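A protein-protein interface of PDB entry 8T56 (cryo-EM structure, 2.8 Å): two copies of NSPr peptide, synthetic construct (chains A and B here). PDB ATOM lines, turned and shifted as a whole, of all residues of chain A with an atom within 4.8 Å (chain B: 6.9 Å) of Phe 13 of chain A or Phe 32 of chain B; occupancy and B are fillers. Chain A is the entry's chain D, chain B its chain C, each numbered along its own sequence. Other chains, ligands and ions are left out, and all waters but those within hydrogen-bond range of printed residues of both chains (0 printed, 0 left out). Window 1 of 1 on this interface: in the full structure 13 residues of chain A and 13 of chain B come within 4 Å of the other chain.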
ATOM      1  N   VAL A   9      24.171   5.498   7.265  1.00  0.00           N
ATOM      2  CA  VAL A   9      23.567   4.574   6.340  1.00  0.00           C
ATOM      3  C   VAL A   9      22.066   4.645   6.460  1.00  0.00           C
ATOM      4  O   VAL A   9      21.375   4.685   5.443  1.00  0.00           O
ATOM      5  CB  VAL A   9      24.041   3.144   6.566  1.00  0.00           C
ATOM      6  CG1 VAL A   9      23.264   2.192   5.678  1.00  0.00           C
ATOM      7  CG2 VAL A   9      25.487   3.053   6.256  1.00  0.00           C
ATOM      8  N   LYS A  10      21.532   4.658   7.678  1.00  0.00           N
ATOM      9  CA  LYS A  10      20.090   4.743   7.823  1.00  0.00           C
ATOM     10  C   LYS A  10      19.526   6.021   7.242  1.00  0.00           C
ATOM     11  O   LYS A  10      18.472   5.988   6.610  1.00  0.00           O
ATOM     12  CB  LYS A  10      19.659   4.671   9.270  1.00  0.00           C
ATOM     13  CG  LYS A  10      19.793   3.328   9.916  1.00  0.00           C
ATOM     14  CD  LYS A  10      19.079   3.296  11.260  1.00  0.00           C
ATOM     15  CE  LYS A  10      19.825   4.094  12.325  1.00  0.00           C
ATOM     16  NZ  LYS A  10      19.147   4.018  13.657  1.00  0.00           N
ATOM     17  N   ASP A  11      20.232   7.135   7.401  1.00  0.00           N
ATOM     18  CA  ASP A  11      19.752   8.401   6.905  1.00  0.00           C
ATOM     19  C   ASP A  11      19.824   8.433   5.401  1.00  0.00           C
ATOM     20  O   ASP A  11      18.917   8.943   4.748  1.00  0.00           O
ATOM     21  CB  ASP A  11      20.594   9.532   7.473  1.00  0.00           C
ATOM     22  CG  ASP A  11      20.391   9.776   8.958  1.00  0.00           C
ATOM     23  OD1 ASP A  11      19.387   9.373   9.483  1.00  0.00           O
ATOM     24  OD2 ASP A  11      21.274  10.346   9.575  1.00  0.00           O
ATOM     25  N   TYR A  12      20.878   7.875   4.815  1.00  0.00           N
ATOM     26  CA  TYR A  12      20.952   7.873   3.377  1.00  0.00           C
ATOM     27  C   TYR A  12      19.818   7.086   2.796  1.00  0.00           C
ATOM     28  O   TYR A  12      19.092   7.559   1.911  1.00  0.00           O
ATOM     29  CB  TYR A  12      22.229   7.269   2.838  1.00  0.00           C
ATOM     30  CG  TYR A  12      22.228   7.292   1.326  1.00  0.00           C
ATOM     31  CD1 TYR A  12      22.646   8.399   0.682  1.00  0.00           C
ATOM     32  CD2 TYR A  12      21.763   6.228   0.599  1.00  0.00           C
ATOM     33  CE1 TYR A  12      22.611   8.450  -0.670  1.00  0.00           C
ATOM     34  CE2 TYR A  12      21.722   6.285  -0.750  1.00  0.00           C
ATOM     35  CZ  TYR A  12      22.145   7.397  -1.379  1.00  0.00           C
ATOM     36  OH  TYR A  12      22.115   7.479  -2.733  1.00  0.00           O
ATOM     37  N   PHE A  13      19.611   5.883   3.302  1.00  0.00           N
ATOM     38  CA  PHE A  13      18.591   5.080   2.695  1.00  0.00           C
ATOM     39  C   PHE A  13      17.206   5.598   2.969  1.00  0.00           C
ATOM     40  O   PHE A  13      16.338   5.525   2.108  1.00  0.00           O
ATOM     41  CB  PHE A  13      18.786   3.623   3.036  1.00  0.00           C
ATOM     42  CG  PHE A  13      19.877   3.064   2.181  1.00  0.00           C
ATOM     43  CD1 PHE A  13      21.139   2.914   2.640  1.00  0.00           C
ATOM     44  CD2 PHE A  13      19.629   2.731   0.887  1.00  0.00           C
ATOM     45  CE1 PHE A  13      22.129   2.447   1.833  1.00  0.00           C
ATOM     46  CE2 PHE A  13      20.613   2.267   0.081  1.00  0.00           C
ATOM     47  CZ  PHE A  13      21.865   2.128   0.556  1.00  0.00           C
ATOM     48  N   ALA A  14      16.961   6.138   4.140  1.00  0.00           N
ATOM     49  CA  ALA A  14      15.650   6.667   4.405  1.00  0.00           C
ATOM     50  C   ALA A  14      15.311   7.897   3.569  1.00  0.00           C
ATOM     51  O   ALA A  14      14.162   8.058   3.162  1.00  0.00           O
ATOM     52  CB  ALA A  14      15.546   7.035   5.860  1.00  0.00           C
ATOM     53  N   LYS A  15      16.290   8.774   3.310  1.00  0.00           N
ATOM     54  CA  LYS A  15      16.000  10.031   2.630  1.00  0.00           C
ATOM     55  C   LYS A  15      16.514  10.269   1.216  1.00  0.00           C
ATOM     56  O   LYS A  15      15.858  10.980   0.461  1.00  0.00           O
ATOM     57  CB  LYS A  15      16.525  11.148   3.502  1.00  0.00           C
ATOM     58  CG  LYS A  15      15.819  11.235   4.818  1.00  0.00           C
ATOM     59  CD  LYS A  15      16.370  12.326   5.678  1.00  0.00           C
ATOM     60  CE  LYS A  15      15.644  12.370   7.012  1.00  0.00           C
ATOM     61  NZ  LYS A  15      16.200  13.409   7.918  1.00  0.00           N
ATOM     62  N   PHE A  16      17.669   9.735   0.838  1.00  0.00           N
ATOM     63  CA  PHE A  16      18.223  10.066  -0.465  1.00  0.00           C
ATOM     64  C   PHE A  16      18.153   8.924  -1.434  1.00  0.00           C
ATOM     65  O   PHE A  16      18.190   9.128  -2.648  1.00  0.00           O
ATOM     66  CB  PHE A  16      19.628  10.557  -0.290  1.00  0.00           C
ATOM     67  CG  PHE A  16      19.612  11.765   0.502  1.00  0.00           C
ATOM     68  CD1 PHE A  16      19.945  11.730   1.806  1.00  0.00           C
ATOM     69  CD2 PHE A  16      19.219  12.947  -0.041  1.00  0.00           C
ATOM     70  CE1 PHE A  16      19.885  12.837   2.561  1.00  0.00           C
ATOM     71  CE2 PHE A  16      19.165  14.059   0.711  1.00  0.00           C
ATOM     72  CZ  PHE A  16      19.493  13.998   2.015  1.00  0.00           C
ATOM     73  N   TRP A  17      17.981   7.727  -0.927  1.00  0.00           N
ATOM     74  CA  TRP A  17      17.874   6.593  -1.808  1.00  0.00           C
ATOM     75  C   TRP A  17      16.748   6.750  -2.790  1.00  0.00           C
ATOM     76  O   TRP A  17      16.952   6.534  -3.973  1.00  0.00           O
ATOM     77  CB  TRP A  17      17.727   5.335  -1.020  1.00  0.00           C
ATOM     78  CG  TRP A  17      17.350   4.162  -1.757  1.00  0.00           C
ATOM     79  CD1 TRP A  17      16.189   3.562  -1.613  1.00  0.00           C
ATOM     80  CD2 TRP A  17      18.057   3.419  -2.737  1.00  0.00           C
ATOM     81  NE1 TRP A  17      16.113   2.504  -2.396  1.00  0.00           N
ATOM     82  CE2 TRP A  17      17.243   2.398  -3.102  1.00  0.00           C
ATOM     83  CE3 TRP A  17      19.296   3.534  -3.320  1.00  0.00           C
ATOM     84  CZ2 TRP A  17      17.608   1.481  -4.031  1.00  0.00           C
ATOM     85  CZ3 TRP A  17      19.665   2.606  -4.257  1.00  0.00           C
ATOM     86  CH2 TRP A  17      18.841   1.611  -4.601  1.00  0.00           C
ATOM     87  N   ALA B  27      12.282  -2.388  -1.711  1.00  0.00           N
ATOM     88  CA  ALA B  27      12.906  -3.470  -0.987  1.00  0.00           C
ATOM     89  C   ALA B  27      14.202  -3.042  -0.333  1.00  0.00           C
ATOM     90  O   ALA B  27      14.486  -3.449   0.793  1.00  0.00           O
ATOM     91  CB  ALA B  27      13.179  -4.616  -1.922  1.00  0.00           C
ATOM     92  N   VAL B  28      14.982  -2.213  -1.015  1.00  0.00           N
ATOM     93  CA  VAL B  28      16.232  -1.751  -0.450  1.00  0.00           C
ATOM     94  C   VAL B  28      16.045  -0.856   0.738  1.00  0.00           C
ATOM     95  O   VAL B  28      16.724  -1.013   1.753  1.00  0.00           O
ATOM     96  CB  VAL B  28      17.046  -1.002  -1.483  1.00  0.00           C
ATOM     97  CG1 VAL B  28      18.234  -0.346  -0.839  1.00  0.00           C
ATOM     98  CG2 VAL B  28      17.506  -1.949  -2.526  1.00  0.00           C
ATOM     99  N   LYS B  29      15.151   0.106   0.615  1.00  0.00           N
ATOM    100  CA  LYS B  29      14.909   1.029   1.689  1.00  0.00           C
ATOM    101  C   LYS B  29      14.418   0.299   2.927  1.00  0.00           C
ATOM    102  O   LYS B  29      14.831   0.597   4.056  1.00  0.00           O
ATOM    103  CB  LYS B  29      13.871   2.022   1.218  1.00  0.00           C
ATOM    104  CG  LYS B  29      13.569   3.136   2.117  1.00  0.00           C
ATOM    105  CD  LYS B  29      12.227   3.699   1.734  1.00  0.00           C
ATOM    106  CE  LYS B  29      12.165   4.066   0.289  1.00  0.00           C
ATOM    107  NZ  LYS B  29      10.892   4.747  -0.029  1.00  0.00           N
ATOM    108  N   ASP B  30      13.553  -0.685   2.705  1.00  0.00           N
ATOM    109  CA  ASP B  30      12.962  -1.458   3.771  1.00  0.00           C
ATOM    110  C   ASP B  30      14.008  -2.329   4.427  1.00  0.00           C
ATOM    111  O   ASP B  30      14.031  -2.454   5.648  1.00  0.00           O
ATOM    112  CB  ASP B  30      11.833  -2.314   3.232  1.00  0.00           C
ATOM    113  CG  ASP B  30      11.059  -3.013   4.287  1.00  0.00           C
ATOM    114  OD1 ASP B  30      10.389  -2.363   5.060  1.00  0.00           O
ATOM    115  OD2 ASP B  30      11.149  -4.214   4.375  1.00  0.00           O
ATOM    116  N   TYR B  31      14.900  -2.911   3.635  1.00  0.00           N
ATOM    117  CA  TYR B  31      15.964  -3.728   4.166  1.00  0.00           C
ATOM    118  C   TYR B  31      16.841  -2.975   5.125  1.00  0.00           C
ATOM    119  O   TYR B  31      17.069  -3.416   6.246  1.00  0.00           O
ATOM    120  CB  TYR B  31      16.820  -4.259   3.036  1.00  0.00           C
ATOM    121  CG  TYR B  31      18.049  -4.957   3.478  1.00  0.00           C
ATOM    122  CD1 TYR B  31      18.004  -6.242   3.927  1.00  0.00           C
ATOM    123  CD2 TYR B  31      19.244  -4.300   3.414  1.00  0.00           C
ATOM    124  CE1 TYR B  31      19.162  -6.865   4.311  1.00  0.00           C
ATOM    125  CE2 TYR B  31      20.394  -4.910   3.793  1.00  0.00           C
ATOM    126  CZ  TYR B  31      20.363  -6.188   4.240  1.00  0.00           C
ATOM    127  OH  TYR B  31      21.524  -6.812   4.624  1.00  0.00           O
ATOM    128  N   PHE B  32      17.308  -1.801   4.733  1.00  0.00           N
ATOM    129  CA  PHE B  32      18.222  -1.097   5.613  1.00  0.00           C
ATOM    130  C   PHE B  32      17.540  -0.634   6.867  1.00  0.00           C
ATOM    131  O   PHE B  32      18.121  -0.687   7.951  1.00  0.00           O
ATOM    132  CB  PHE B  32      18.897   0.048   4.895  1.00  0.00           C
ATOM    133  CG  PHE B  32      20.008  -0.425   4.079  1.00  0.00           C
ATOM    134  CD1 PHE B  32      19.878  -0.635   2.749  1.00  0.00           C
ATOM    135  CD2 PHE B  32      21.202  -0.674   4.662  1.00  0.00           C
ATOM    136  CE1 PHE B  32      20.926  -1.092   2.018  1.00  0.00           C
ATOM    137  CE2 PHE B  32      22.250  -1.126   3.940  1.00  0.00           C
ATOM    138  CZ  PHE B  32      22.109  -1.336   2.616  1.00  0.00           C
ATOM    139  N   ALA B  33      16.271  -0.292   6.762  1.00  0.00           N
ATOM    140  CA  ALA B  33      15.481   0.167   7.885  1.00  0.00           C
ATOM    141  C   ALA B  33      15.318  -0.892   8.973  1.00  0.00           C
ATOM    142  O   ALA B  33      14.910  -0.567  10.088  1.00  0.00           O
ATOM    143  CB  ALA B  33      14.114   0.586   7.406  1.00  0.00           C
ATOM    144  N   LYS B  34      15.543  -2.164   8.643  1.00  0.00           N
ATOM    145  CA  LYS B  34      15.374  -3.254   9.588  1.00  0.00           C
ATOM    146  C   LYS B  34      16.665  -3.806  10.158  1.00  0.00           C
ATOM    147  O   LYS B  34      16.629  -4.689  11.012  1.00  0.00           O
ATOM    148  CB  LYS B  34      14.623  -4.412   8.949  1.00  0.00           C
ATOM    149  CG  LYS B  34      13.185  -4.141   8.650  1.00  0.00           C
ATOM    150  CD  LYS B  34      12.519  -5.387   8.073  1.00  0.00           C
ATOM    151  CE  LYS B  34      10.998  -5.260   8.051  1.00  0.00           C
ATOM    152  NZ  LYS B  34      10.533  -4.283   7.058  1.00  0.00           N
ATOM    153  N   LEU B  35      17.810  -3.334   9.704  1.00  0.00           N
ATOM    154  CA  LEU B  35      19.037  -3.958  10.187  1.00  0.00           C
ATOM    155  C   LEU B  35      19.431  -3.702  11.629  1.00  0.00           C
ATOM    156  O   LEU B  35      20.099  -4.560  12.212  1.00  0.00           O
ATOM    157  CB  LEU B  35      20.232  -3.573   9.311  1.00  0.00           C
ATOM    158  CG  LEU B  35      20.286  -4.135   7.901  1.00  0.00           C
ATOM    159  CD1 LEU B  35      21.427  -3.468   7.190  1.00  0.00           C
ATOM    160  CD2 LEU B  35      20.499  -5.646   7.938  1.00  0.00           C
ATOM    161  N   TRP B  36      19.068  -2.530  12.215  1.00  0.00           N
ATOM    162  CA  TRP B  36      19.510  -2.162  13.561  1.00  0.00           C
ATOM    163  C   TRP B  36      18.310  -1.648  14.332  1.00  0.00           C
ATOM    164  O   TRP B  36      18.375  -1.425  15.543  1.00  0.00           O
ATOM    165  CB  TRP B  36      20.649  -1.094  13.492  1.00  0.00           C
ATOM    166  CG  TRP B  36      21.828  -1.520  12.545  1.00  0.00           C
ATOM    167  CD1 TRP B  36      22.792  -2.482  12.766  1.00  0.00           C
ATOM    168  CD2 TRP B  36      22.117  -0.960  11.250  1.00  0.00           C
ATOM    169  NE1 TRP B  36      23.639  -2.578  11.692  1.00  0.00           N
ATOM    170  CE2 TRP B  36      23.262  -1.659  10.748  1.00  0.00           C
ATOM    171  CE3 TRP B  36      21.492   0.112  10.423  1.00  0.00           C
ATOM    172  CZ2 TRP B  36      23.842  -1.351   9.435  1.00  0.00           C
ATOM    173  CZ3 TRP B  36      22.075   0.430   9.106  1.00  0.00           C
ATOM    174  CH2 TRP B  36      23.224  -0.290   8.633  1.00  0.00           C
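No position is printed for both chains.
Of the 8 pairs that touch across the chains among the printed residues, none has its exchanged pair printed and touching as well.
Of the 9 printed residues of chain A, 4 touch a printed residue of chain B.
Among the printed residues, 8 pairs touch across the chains.
Among the printed residues, no Asp or Glu carboxylate lies within 4 Å of a Lys or Arg side-chain nitrogen of the other chain.
Of the printed residues of chain B, Lys 10 of chain A touches Trp 36.
Of chain B, only Val 28 (3.7 Å), Lys 29 (3.7 Å) and Phe 32 (3.7 Å) come within 4 Å of Phe 13 of chain A.
Lys 15 of chain A touches none of the printed residues of chain B.
Printed residues of chain B within 4 Å of Trp 17 of chain A: Val 28 and Lys 29.
Ala 27 of chain B touches none of the printed residues of chain A.
Printed residues of chain A within 4 Å of Phe 32 of chain B: Val 9 (3.7 Å) and Phe 13 (3.7 Å).
Printed residues of chain A within 4 Å of Trp 36 of chain B: Val 9 (3.9 Å) and Lys 10 (3.7 Å).
The nearest printed residue of chain A that does not touch Trp 36 of chain B is Phe 13 of chain A (7.0 Å).
The backbone carbonyl oxygen of Tyr 12 of chain A sits at hydrogen-bond distance from the backbone NH of Trp 17 of chain A.
Phe 32 of chain B touches Val 9 of chain A.
Trp 36 of chain B touches Val 9 of chain A.
Lys 10 of chain A touches Trp 36 of chain B (CG to CE3, 3.7 Å).
Val 28 of chain B touches Phe 13 of chain A.
O of Phe 13 of chain A touches CG of Lys 29 of chain B, 3.7 Å away.
Phe 32 of chain B touches Phe 13 of chain A (CE1 to CZ, 3.7 Å).
Trp 17 of chain A touches Val 28 of chain B.
N of Lys 29 of chain B touches NE1 of Trp 17 of chain A, at 3.97 Å.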
